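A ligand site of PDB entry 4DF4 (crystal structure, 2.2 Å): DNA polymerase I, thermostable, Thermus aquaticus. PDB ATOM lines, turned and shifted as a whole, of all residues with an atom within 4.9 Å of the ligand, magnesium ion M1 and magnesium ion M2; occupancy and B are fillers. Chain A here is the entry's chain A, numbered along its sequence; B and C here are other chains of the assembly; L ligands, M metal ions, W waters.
An oxygen (O3) of the ligand is in salt-bridge range of the guanidinium group (NH1) of Arg 367.
N4 of the ligand is in hydrogen-bond range of O4 of DT 4 of chain B, at 2.6 Å.
NZ of Lys 371 is in salt-bridge range of O3 of the ligand, 2.7 Å away.
N5 of the ligand sits at hydrogen-bond distance from OP2 of DOC 12 of chain C (3.0 Å).
An oxygen (O1) of the ligand sits at hydrogen-bond distance from the backbone NH of Gln 321 (3.1 Å).
A ring nitrogen (NE2) of His 347 sits at hydrogen-bond distance from an oxygen (O5) of the ligand, at 3.1 Å.
The backbone NH of Glu 323 lies within hydrogen-bond range of an oxygen (O11) of the ligand (3.1 Å).
The guanidinium group (NH2) of Arg 281 is in hydrogen-bond range of an oxygen (O12) of the ligand (3.2 Å).
OD1 of Asp 493 binds magnesium ion M2 (2.1 Å).
OD2 of Asp 318 is bound to magnesium ion M2 (2.2 Å).
Magnesium ion M2 is bound by O8 of the ligand, at 2.2 Å.
Magnesium ion M2 has three donor atoms within binding distance.
Slightly farther from magnesium ion M2 lies water W1 (2.8 Å).
DOC 12 of chain C touches magnesium ion M2.
Within 4 Å of magnesium ion M2: Asp 318, Asp 493 and DOC 12 of chain C.
The nearest printed residue that does not touch magnesium ion M2 is Glu 494 (4.5 Å).
O2 of DOC 12 of chain C is in hydrogen-bond range of NH1 of Arg 281 (2.7 Å).
OP2 of DOC 12 of chain C lies within salt-bridge range of the guanidinium group of Arg 368, 3.0 Å away.
N2 of DG 5 of chain B lies close to O2 of DOC 12 of chain C (2.6 Å).
The side-chain amide nitrogen (NE2) of Gln 321 lies within hydrogen-bond range of the side-chain hydroxyl (OG) of Ser 320, 3.4 Å away.
The guanidinium group (NH2) of Arg 281 lies within salt-bridge range of the side-chain carboxylate (OE2) of Glu 323 (3.7 Å).
OH of Tyr 379 is in hydrogen-bond range of OE1 of Glu 323 (2.6 Å).
The guanidinium group of Arg 281 is in hydrogen-bond range of N2 of DG 5 of chain B (3.5 Å).
The nearest printed residue that does not touch magnesium ion M1 is Ser 320 (4.2 Å).
Ser 320 touches the ligand.
Ile 322 touches the ligand (CG2 to O11, 3.3 Å).
CG of Arg 368 touches O13 of the ligand, at 3.2 Å.
CZ of Phe 375 touches O5 of the ligand (3.1 Å).
DG 5 of chain B touches the ligand.
Hydrophobic or aromatic side chains within 4 Å of the ligand: Ile 322, His 347 and Phe 375.
Within 4 Å of the ligand: Arg 281, Asp 318, Tyr 319, Ser 320, Gln 321, Ile 322, Glu 323, His 347, Arg 367, Arg 368, Lys 371, Phe 375, Asp 493, DT 4 of chain B, DG 5 of chain B and DOC 12 of chain C.
The nearest printed residue that does not touch the ligand is Tyr 379 (4.01 Å).
Water W1 bridges a nitrogen (N5) of the ligand (3.0 Å) and O5' of DOC 12 of chain C (3.4 Å).
Water W4 bridges O of Asp 318 (3.2 Å) and O1 of the ligand (3.4 Å).
Water W3 bridges the side-chain amino group of Lys 371 and an oxygen (O3) of the ligand.
Magnesium ion M1 is bound by the backbone carbonyl oxygen of Tyr 319 (2.0 Å), the side-chain carboxylate of Asp 318 (2.0 Å), an oxygen (O2) of the ligand (2.0 Å), the side-chain carboxylate of Asp 493 (2.0 Å), an oxygen (O6) of the ligand (2.1 Å) and an oxygen (O8) of the ligand (2.1 Å).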
ATOM      1  N   ARG A 281      35.901   2.224  26.559  1.00  0.00           N
ATOM      2  CA  ARG A 281      35.259   3.069  27.556  1.00  0.00           C
ATOM      3  C   ARG A 281      36.287   3.519  28.592  1.00  0.00           C
ATOM      4  O   ARG A 281      37.317   2.887  28.773  1.00  0.00           O
ATOM      5  CB  ARG A 281      34.148   2.304  28.275  1.00  0.00           C
ATOM      6  CG  ARG A 281      32.789   2.351  27.618  1.00  0.00           C
ATOM      7  CD  ARG A 281      31.731   1.805  28.569  1.00  0.00           C
ATOM      8  NE  ARG A 281      30.376   1.966  28.046  1.00  0.00           N
ATOM      9  CZ  ARG A 281      29.276   1.681  28.730  1.00  0.00           C
ATOM     10  NH1 ARG A 281      29.373   1.228  29.977  1.00  0.00           N
ATOM     11  NH2 ARG A 281      28.084   1.852  28.176  1.00  0.00           N
ATOM     12  N   VAL A 294      20.577   6.447  41.073  1.00  0.00           N
ATOM     13  CA  VAL A 294      19.629   7.341  40.413  1.00  0.00           C
ATOM     14  C   VAL A 294      18.259   6.679  40.246  1.00  0.00           C
ATOM     15  O   VAL A 294      17.267   7.351  39.956  1.00  0.00           O
ATOM     16  CB  VAL A 294      20.161   7.792  39.042  1.00  0.00           C
ATOM     17  CG1 VAL A 294      19.967   6.683  38.013  1.00  0.00           C
ATOM     18  CG2 VAL A 294      19.484   9.070  38.588  1.00  0.00           C
ATOM     19  N   ASP A 318      23.237  14.225  27.872  1.00  0.00           N
ATOM     20  CA  ASP A 318      23.184  12.785  27.651  1.00  0.00           C
ATOM     21  C   ASP A 318      22.790  12.466  26.216  1.00  0.00           C
ATOM     22  O   ASP A 318      21.796  12.982  25.707  1.00  0.00           O
ATOM     23  CB  ASP A 318      22.227  12.113  28.648  1.00  0.00           C
ATOM     24  CG  ASP A 318      22.368  10.585  28.670  1.00  0.00           C
ATOM     25  OD1 ASP A 318      22.504   9.974  27.596  1.00  0.00           O
ATOM     26  OD2 ASP A 318      22.333   9.985  29.762  1.00  0.00           O
ATOM     27  N   TYR A 319      23.564  11.604  25.568  1.00  0.00           N
ATOM     28  CA  TYR A 319      23.262  11.152  24.212  1.00  0.00           C
ATOM     29  C   TYR A 319      21.997  10.306  24.225  1.00  0.00           C
ATOM     30  O   TYR A 319      21.827   9.446  25.088  1.00  0.00           O
ATOM     31  CB  TYR A 319      24.411  10.333  23.644  1.00  0.00           C
ATOM     32  CG  TYR A 319      25.528  11.143  23.017  1.00  0.00           C
ATOM     33  CD1 TYR A 319      25.348  11.791  21.803  1.00  0.00           C
ATOM     34  CD2 TYR A 319      26.771  11.246  23.631  1.00  0.00           C
ATOM     35  CE1 TYR A 319      26.363  12.521  21.214  1.00  0.00           C
ATOM     36  CE2 TYR A 319      27.797  11.980  23.059  1.00  0.00           C
ATOM     37  CZ  TYR A 319      27.592  12.613  21.852  1.00  0.00           C
ATOM     38  OH  TYR A 319      28.609  13.341  21.287  1.00  0.00           O
ATOM     39  N   SER A 320      21.121  10.536  23.250  1.00  0.00           N
ATOM     40  CA  SER A 320      19.880   9.779  23.163  1.00  0.00           C
ATOM     41  C   SER A 320      20.056   8.480  22.394  1.00  0.00           C
ATOM     42  O   SER A 320      20.466   8.486  21.226  1.00  0.00           O
ATOM     43  CB  SER A 320      18.784  10.618  22.503  1.00  0.00           C
ATOM     44  OG  SER A 320      17.668   9.817  22.167  1.00  0.00           O
ATOM     45  N   GLN A 321      19.744   7.356  23.045  1.00  0.00           N
ATOM     46  CA  GLN A 321      19.753   6.028  22.425  1.00  0.00           C
ATOM     47  C   GLN A 321      21.030   5.758  21.644  1.00  0.00           C
ATOM     48  O   GLN A 321      20.983   5.196  20.549  1.00  0.00           O
ATOM     49  CB  GLN A 321      18.551   5.877  21.496  1.00  0.00           C
ATOM     50  CG  GLN A 321      17.244   6.430  22.045  1.00  0.00           C
ATOM     51  CD  GLN A 321      16.133   6.425  21.017  1.00  0.00           C
ATOM     52  OE1 GLN A 321      15.672   5.361  20.591  1.00  0.00           O
ATOM     53  NE2 GLN A 321      15.692   7.610  20.601  1.00  0.00           N
ATOM     54  N   ILE A 322      22.158   6.159  22.208  1.00  0.00           N
ATOM     55  CA  ILE A 322      23.416   6.237  21.461  1.00  0.00           C
ATOM     56  C   ILE A 322      23.861   4.935  20.780  1.00  0.00           C
ATOM     57  O   ILE A 322      24.222   4.953  19.602  1.00  0.00           O
ATOM     58  CB  ILE A 322      24.569   6.834  22.329  1.00  0.00           C
ATOM     59  CG1 ILE A 322      25.839   6.985  21.492  1.00  0.00           C
ATOM     60  CG2 ILE A 322      24.823   5.980  23.568  1.00  0.00           C
ATOM     61  CD1 ILE A 322      25.682   7.933  20.311  1.00  0.00           C
ATOM     62  N   GLU A 323      23.810   3.820  21.495  1.00  0.00           N
ATOM     63  CA  GLU A 323      24.303   2.568  20.940  1.00  0.00           C
ATOM     64  C   GLU A 323      23.378   1.967  19.882  1.00  0.00           C
ATOM     65  O   GLU A 323      23.816   1.203  19.027  1.00  0.00           O
ATOM     66  CB  GLU A 323      24.624   1.550  22.051  1.00  0.00           C
ATOM     67  CG  GLU A 323      25.822   1.970  22.893  1.00  0.00           C
ATOM     68  CD  GLU A 323      26.374   0.854  23.767  1.00  0.00           C
ATOM     69  OE1 GLU A 323      25.951  -0.316  23.590  1.00  0.00           O
ATOM     70  OE2 GLU A 323      27.232   1.144  24.628  1.00  0.00           O
ATOM     71  N   LEU A 324      22.101   2.341  19.930  1.00  0.00           N
ATOM     72  CA  LEU A 324      21.155   1.932  18.890  1.00  0.00           C
ATOM     73  C   LEU A 324      21.426   2.707  17.601  1.00  0.00           C
ATOM     74  O   LEU A 324      21.358   2.157  16.502  1.00  0.00           O
ATOM     75  CB  LEU A 324      19.709   2.146  19.344  1.00  0.00           C
ATOM     76  CG  LEU A 324      19.207   1.247  20.474  1.00  0.00           C
ATOM     77  CD1 LEU A 324      17.725   1.449  20.710  1.00  0.00           C
ATOM     78  CD2 LEU A 324      19.510  -0.215  20.182  1.00  0.00           C
ATOM     79  N   HIS A 347      13.162   2.895  22.879  1.00  0.00           N
ATOM     80  CA  HIS A 347      13.014   2.700  24.325  1.00  0.00           C
ATOM     81  C   HIS A 347      11.585   2.965  24.778  1.00  0.00           C
ATOM     82  O   HIS A 347      11.000   2.173  25.529  1.00  0.00           O
ATOM     83  CB  HIS A 347      13.993   3.582  25.087  1.00  0.00           C
ATOM     84  CG  HIS A 347      15.430   3.217  24.889  1.00  0.00           C
ATOM     85  ND1 HIS A 347      15.829   1.972  24.463  1.00  0.00           N
ATOM     86  CD2 HIS A 347      16.564   3.937  25.042  1.00  0.00           C
ATOM     87  CE1 HIS A 347      17.150   1.933  24.377  1.00  0.00           C
ATOM     88  NE2 HIS A 347      17.618   3.124  24.714  1.00  0.00           N
ATOM     89  N   ARG A 367      10.868   3.562  31.158  1.00  0.00           N
ATOM     90  CA  ARG A 367      11.784   3.676  30.032  1.00  0.00           C
ATOM     91  C   ARG A 367      13.132   3.045  30.390  1.00  0.00           C
ATOM     92  O   ARG A 367      13.830   2.520  29.522  1.00  0.00           O
ATOM     93  CB  ARG A 367      11.969   5.140  29.642  1.00  0.00           C
ATOM     94  CG  ARG A 367      12.653   5.356  28.303  1.00  0.00           C
ATOM     95  CD  ARG A 367      12.738   6.831  27.961  1.00  0.00           C
ATOM     96  NE  ARG A 367      13.347   7.058  26.653  1.00  0.00           N
ATOM     97  CZ  ARG A 367      14.655   7.137  26.445  1.00  0.00           C
ATOM     98  NH1 ARG A 367      15.494   7.013  27.461  1.00  0.00           N
ATOM     99  NH2 ARG A 367      15.123   7.339  25.220  1.00  0.00           N
ATOM    100  N   ARG A 368      13.487   3.106  31.668  1.00  0.00           N
ATOM    101  CA  ARG A 368      14.710   2.489  32.161  1.00  0.00           C
ATOM    102  C   ARG A 368      14.652   0.975  32.000  1.00  0.00           C
ATOM    103  O   ARG A 368      15.627   0.355  31.557  1.00  0.00           O
ATOM    104  CB  ARG A 368      14.924   2.837  33.639  1.00  0.00           C
ATOM    105  CG  ARG A 368      16.138   2.163  34.263  1.00  0.00           C
ATOM    106  CD  ARG A 368      16.247   2.472  35.744  1.00  0.00           C
ATOM    107  NE  ARG A 368      17.499   1.998  36.312  1.00  0.00           N
ATOM    108  CZ  ARG A 368      18.605   2.732  36.405  1.00  0.00           C
ATOM    109  NH1 ARG A 368      18.616   3.973  35.957  1.00  0.00           N
ATOM    110  NH2 ARG A 368      19.704   2.210  36.936  1.00  0.00           N
ATOM    111  N   LYS A 371      15.253  -0.361  28.538  1.00  0.00           N
ATOM    112  CA  LYS A 371      16.645  -0.393  28.090  1.00  0.00           C
ATOM    113  C   LYS A 371      17.258  -1.772  28.309  1.00  0.00           C
ATOM    114  O   LYS A 371      18.043  -2.240  27.480  1.00  0.00           O
ATOM    115  CB  LYS A 371      17.467   0.662  28.827  1.00  0.00           C
ATOM    116  CG  LYS A 371      17.041   2.090  28.550  1.00  0.00           C
ATOM    117  CD  LYS A 371      18.008   3.076  29.156  1.00  0.00           C
ATOM    118  CE  LYS A 371      17.517   4.495  29.031  1.00  0.00           C
ATOM    119  NZ  LYS A 371      18.481   5.475  29.592  1.00  0.00           N
ATOM    120  N   THR A 372      16.907  -2.406  29.426  1.00  0.00           N
ATOM    121  CA  THR A 372      17.377  -3.760  29.716  1.00  0.00           C
ATOM    122  C   THR A 372      16.910  -4.713  28.630  1.00  0.00           C
ATOM    123  O   THR A 372      17.667  -5.588  28.202  1.00  0.00           O
ATOM    124  CB  THR A 372      16.858  -4.244  31.089  1.00  0.00           C
ATOM    125  OG1 THR A 372      17.308  -3.362  32.120  1.00  0.00           O
ATOM    126  CG2 THR A 372      17.355  -5.656  31.377  1.00  0.00           C
ATOM    127  N   PHE A 375      18.574  -3.589  24.853  1.00  0.00           N
ATOM    128  CA  PHE A 375      20.007  -3.885  24.783  1.00  0.00           C
ATOM    129  C   PHE A 375      20.281  -5.350  25.106  1.00  0.00           C
ATOM    130  O   PHE A 375      21.176  -5.956  24.526  1.00  0.00           O
ATOM    131  CB  PHE A 375      20.785  -2.965  25.720  1.00  0.00           C
ATOM    132  CG  PHE A 375      20.663  -1.515  25.380  1.00  0.00           C
ATOM    133  CD1 PHE A 375      20.776  -1.096  24.061  1.00  0.00           C
ATOM    134  CD2 PHE A 375      20.424  -0.569  26.363  1.00  0.00           C
ATOM    135  CE1 PHE A 375      20.655   0.239  23.730  1.00  0.00           C
ATOM    136  CE2 PHE A 375      20.294   0.768  26.036  1.00  0.00           C
ATOM    137  CZ  PHE A 375      20.418   1.168  24.727  1.00  0.00           C
ATOM    138  N   TYR A 379      22.033  -7.872  22.490  1.00  0.00           N
ATOM    139  CA  TYR A 379      23.318  -8.463  22.816  1.00  0.00           C
ATOM    140  C   TYR A 379      23.220  -9.940  23.203  1.00  0.00           C
ATOM    141  O   TYR A 379      24.081 -10.462  23.908  1.00  0.00           O
ATOM    142  CB  TYR A 379      24.023  -7.640  23.898  1.00  0.00           C
ATOM    143  CG  TYR A 379      24.355  -6.239  23.447  1.00  0.00           C
ATOM    144  CD1 TYR A 379      24.850  -6.000  22.159  1.00  0.00           C
ATOM    145  CD2 TYR A 379      24.155  -5.150  24.279  1.00  0.00           C
ATOM    146  CE1 TYR A 379      25.147  -4.722  21.740  1.00  0.00           C
ATOM    147  CE2 TYR A 379      24.445  -3.861  23.861  1.00  0.00           C
ATOM    148  CZ  TYR A 379      24.948  -3.659  22.591  1.00  0.00           C
ATOM    149  OH  TYR A 379      25.245  -2.382  22.172  1.00  0.00           O
ATOM    150  N   VAL A 491      29.989  10.052  32.242  1.00  0.00           N
ATOM    151  CA  VAL A 491      29.353   8.771  32.557  1.00  0.00           C
ATOM    152  C   VAL A 491      29.006   8.032  31.251  1.00  0.00           C
ATOM    153  O   VAL A 491      27.832   7.847  30.933  1.00  0.00           O
ATOM    154  CB  VAL A 491      28.095   8.937  33.441  1.00  0.00           C
ATOM    155  CG1 VAL A 491      27.701   7.602  34.046  1.00  0.00           C
ATOM    156  CG2 VAL A 491      28.355   9.955  34.540  1.00  0.00           C
ATOM    157  N   ASP A 493      28.023   7.876  28.245  1.00  0.00           N
ATOM    158  CA  ASP A 493      27.387   8.699  27.217  1.00  0.00           C
ATOM    159  C   ASP A 493      26.838   9.987  27.822  1.00  0.00           C
ATOM    160  O   ASP A 493      26.009  10.668  27.210  1.00  0.00           O
ATOM    161  CB  ASP A 493      26.337   7.927  26.408  1.00  0.00           C
ATOM    162  CG  ASP A 493      24.999   7.804  27.121  1.00  0.00           C
ATOM    163  OD1 ASP A 493      24.948   7.824  28.373  1.00  0.00           O
ATOM    164  OD2 ASP A 493      23.980   7.654  26.405  1.00  0.00           O
ATOM    165  N   GLU A 494      27.314  10.310  29.009  1.00  0.00           N
ATOM    166  CA  GLU A 494      26.867  11.502  29.711  1.00  0.00           C
ATOM    167  C   GLU A 494      28.049  12.419  30.032  1.00  0.00           C
ATOM    168  O   GLU A 494      29.147  11.952  30.305  1.00  0.00           O
ATOM    169  CB  GLU A 494      26.126  11.100  30.992  1.00  0.00           C
ATOM    170  CG  GLU A 494      25.613  12.277  31.801  1.00  0.00           C
ATOM    171  CD  GLU A 494      24.867  11.850  33.044  1.00  0.00           C
ATOM    172  OE1 GLU A 494      24.408  10.688  33.106  1.00  0.00           O
ATOM    173  OE2 GLU A 494      24.745  12.681  33.962  1.00  0.00           O
ATOM    174  P    DT B   4      21.545 -14.621  29.124  1.00  0.00           P
ATOM    175  OP1  DT B   4      21.206 -14.391  30.544  1.00  0.00           O
ATOM    176  OP2  DT B   4      20.654 -15.433  28.263  1.00  0.00           O
ATOM    177  O5'  DT B   4      21.754 -13.197  28.403  1.00  0.00           O
ATOM    178  C5'  DT B   4      22.788 -12.330  28.855  1.00  0.00           C
ATOM    179  C4'  DT B   4      23.290 -11.464  27.722  1.00  0.00           C
ATOM    180  O4'  DT B   4      22.296 -10.468  27.378  1.00  0.00           O
ATOM    181  C3'  DT B   4      24.538 -10.659  28.059  1.00  0.00           C
ATOM    182  O3'  DT B   4      25.690 -11.434  27.781  1.00  0.00           O
ATOM    183  C2'  DT B   4      24.422  -9.482  27.102  1.00  0.00           C
ATOM    184  C1'  DT B   4      22.912  -9.235  27.101  1.00  0.00           C
ATOM    185  N1   DT B   4      22.460  -8.237  28.116  1.00  0.00           N
ATOM    186  C2   DT B   4      22.723  -6.899  27.907  1.00  0.00           C
ATOM    187  O2   DT B   4      23.309  -6.483  26.925  1.00  0.00           O
ATOM    188  N3   DT B   4      22.266  -6.059  28.899  1.00  0.00           N
ATOM    189  C4   DT B   4      21.599  -6.423  30.051  1.00  0.00           C
ATOM    190  O4   DT B   4      21.224  -5.594  30.872  1.00  0.00           O
ATOM    191  C5   DT B   4      21.354  -7.837  30.209  1.00  0.00           C
ATOM    192  C7   DT B   4      20.637  -8.343  31.421  1.00  0.00           C
ATOM    193  C6   DT B   4      21.797  -8.663  29.247  1.00  0.00           C
ATOM    194  P    DG B   5      26.950 -11.396  28.778  1.00  0.00           P
ATOM    195  OP1  DG B   5      27.832 -12.542  28.447  1.00  0.00           O
ATOM    196  OP2  DG B   5      26.446 -11.227  30.149  1.00  0.00           O
ATOM    197  O5'  DG B   5      27.701 -10.047  28.371  1.00  0.00           O
ATOM    198  C5'  DG B   5      28.204  -9.898  27.044  1.00  0.00           C
ATOM    199  C4'  DG B   5      28.504  -8.438  26.740  1.00  0.00           C
ATOM    200  O4'  DG B   5      27.280  -7.659  26.857  1.00  0.00           O
ATOM    201  C3'  DG B   5      29.468  -7.764  27.692  1.00  0.00           C
ATOM    202  O3'  DG B   5      30.808  -8.003  27.276  1.00  0.00           O
ATOM    203  C2'  DG B   5      29.096  -6.295  27.515  1.00  0.00           C
ATOM    204  C1'  DG B   5      27.587  -6.360  27.311  1.00  0.00           C
ATOM    205  N9   DG B   5      26.835  -6.095  28.531  1.00  0.00           N
ATOM    206  C8   DG B   5      26.130  -6.993  29.301  1.00  0.00           C
ATOM    207  N7   DG B   5      25.549  -6.445  30.332  1.00  0.00           N
ATOM    208  C5   DG B   5      25.885  -5.097  30.233  1.00  0.00           C
ATOM    209  C6   DG B   5      25.536  -4.007  31.072  1.00  0.00           C
ATOM    210  O6   DG B   5      24.850  -4.016  32.098  1.00  0.00           O
ATOM    211  N1   DG B   5      26.086  -2.814  30.605  1.00  0.00           N
ATOM    212  C2   DG B   5      26.869  -2.681  29.483  1.00  0.00           C
ATOM    213  N2   DG B   5      27.310  -1.446  29.206  1.00  0.00           N
ATOM    214  N3   DG B   5      27.199  -3.696  28.694  1.00  0.00           N
ATOM    215  C4   DG B   5      26.675  -4.863  29.126  1.00  0.00           C
ATOM    216  N1  DOC C  12      25.340   1.951  32.131  1.00  0.00           N
ATOM    217  C2  DOC C  12      25.750   0.715  31.586  1.00  0.00           C
ATOM    218  N3  DOC C  12      25.100  -0.499  31.989  1.00  0.00           N
ATOM    219  C4  DOC C  12      24.051  -0.461  32.924  1.00  0.00           C
ATOM    220  C5  DOC C  12      23.638   0.780  33.481  1.00  0.00           C
ATOM    221  C6  DOC C  12      24.273   1.986  33.078  1.00  0.00           C
ATOM    222  O2  DOC C  12      26.788   0.661  30.662  1.00  0.00           O
ATOM    223  N4  DOC C  12      23.402  -1.699  33.321  1.00  0.00           N
ATOM    224  C1' DOC C  12      26.027   3.206  31.705  1.00  0.00           C
ATOM    225  C2' DOC C  12      25.493   3.785  30.465  1.00  0.00           C
ATOM    226  C3' DOC C  12      24.634   4.910  30.922  1.00  0.00           C
ATOM    227  C4' DOC C  12      25.345   5.334  32.177  1.00  0.00           C
ATOM    228  O4' DOC C  12      25.925   4.182  32.703  1.00  0.00           O
ATOM    229  C5' DOC C  12      24.408   5.939  33.146  1.00  0.00           C
ATOM    230  O5' DOC C  12      23.467   5.022  33.548  1.00  0.00           O
ATOM    231  P   DOC C  12      22.573   5.344  34.754  1.00  0.00           P
ATOM    232  OP1 DOC C  12      22.272   6.779  35.089  1.00  0.00           O
ATOM    233  OP2 DOC C  12      21.382   4.501  35.060  1.00  0.00           O
HETATM  234  O1  LIG L   1      17.903   8.218  25.331  1.00  0.00           O
HETATM  235  P1  LIG L   1      18.690   7.569  26.445  1.00  0.00           P
HETATM  236  O2  LIG L   1      20.061   8.157  26.706  1.00  0.00           O
HETATM  237  O3  LIG L   1      17.882   7.327  27.699  1.00  0.00           O
HETATM  238  O4  LIG L   1      19.009   6.090  25.882  1.00  0.00           O
HETATM  239  P2  LIG L   1      20.488   5.463  25.951  1.00  0.00           P
HETATM  240  O5  LIG L   1      20.492   4.255  25.045  1.00  0.00           O
HETATM  241  O6  LIG L   1      21.535   6.534  25.742  1.00  0.00           O
HETATM  242  O7  LIG L   1      20.536   4.925  27.471  1.00  0.00           O
HETATM  243  P3  LIG L   1      21.745   5.357  28.436  1.00  0.00           P
HETATM  244  O8  LIG L   1      22.225   6.733  28.033  1.00  0.00           O
HETATM  245  O9  LIG L   1      21.315   5.094  29.860  1.00  0.00           O
HETATM  246  O10 LIG L   1      22.838   4.243  28.037  1.00  0.00           O
HETATM  247  C1  LIG L   1      24.039   4.595  27.367  1.00  0.00           C
HETATM  248  C2  LIG L   1      24.514   3.357  26.613  1.00  0.00           C
HETATM  249  C3  LIG L   1      23.382   2.734  25.824  1.00  0.00           C
HETATM  250  O11 LIG L   1      23.271   3.259  24.505  1.00  0.00           O
HETATM  251  C4  LIG L   1      23.729   1.258  25.800  1.00  0.00           C
HETATM  252  O12 LIG L   1      24.956   2.346  27.525  1.00  0.00           O
HETATM  253  C5  LIG L   1      24.582   1.058  27.048  1.00  0.00           C
HETATM  254  N1  LIG L   1      23.733   0.384  28.051  1.00  0.00           N
HETATM  255  C6  LIG L   1      23.601  -0.958  28.154  1.00  0.00           C
HETATM  256  N2  LIG L   1      24.137  -2.018  27.493  1.00  0.00           N
HETATM  257  C7  LIG L   1      23.816  -3.285  27.814  1.00  0.00           C
HETATM  258  N3  LIG L   1      22.967  -3.620  28.804  1.00  0.00           N
HETATM  259  C8  LIG L   1      22.357  -2.686  29.561  1.00  0.00           C
HETATM  260  N4  LIG L   1      21.500  -3.017  30.555  1.00  0.00           N
HETATM  261  C9  LIG L   1      22.661  -1.264  29.242  1.00  0.00           C
HETATM  262  C10 LIG L   1      22.968   1.031  28.962  1.00  0.00           C
HETATM  263  C11 LIG L   1      22.301   0.083  29.699  1.00  0.00           C
HETATM  264  C12 LIG L   1      21.467   0.334  30.706  1.00  0.00           C
HETATM  265  C13 LIG L   1      20.711   0.559  31.587  1.00  0.00           C
HETATM  266  C14 LIG L   1      19.790   0.805  32.723  1.00  0.00           C
HETATM  267  C15 LIG L   1      19.881   2.228  33.228  1.00  0.00           C
HETATM  268  C16 LIG L   1      19.999   3.244  32.099  1.00  0.00           C
HETATM  269  N5  LIG L   1      19.773   4.615  32.551  1.00  0.00           N
HETATM  270  C17 LIG L   1      18.545   5.056  32.827  1.00  0.00           C
HETATM  271  O13 LIG L   1      17.542   4.472  32.480  1.00  0.00           O
HETATM  272  C18 LIG L   1      18.441   6.347  33.602  1.00  0.00           C
HETATM  273 MG    MG M   1      22.053   8.300  26.659  1.00  0.00          MG
HETATM  274 MG    MG M   2      23.204   7.983  29.611  1.00  0.00          MG
HETATM  275  O   HOH W   1      21.420   6.799  31.417  1.00  0.00           O
HETATM  276  O   HOH W   2      27.055  -1.862  25.734  1.00  0.00           O
HETATM  277  O   HOH W   3      20.240   8.436  30.010  1.00  0.00           O
HETATM  278  O   HOH W   4      19.531  10.929  26.594  1.00  0.00           O
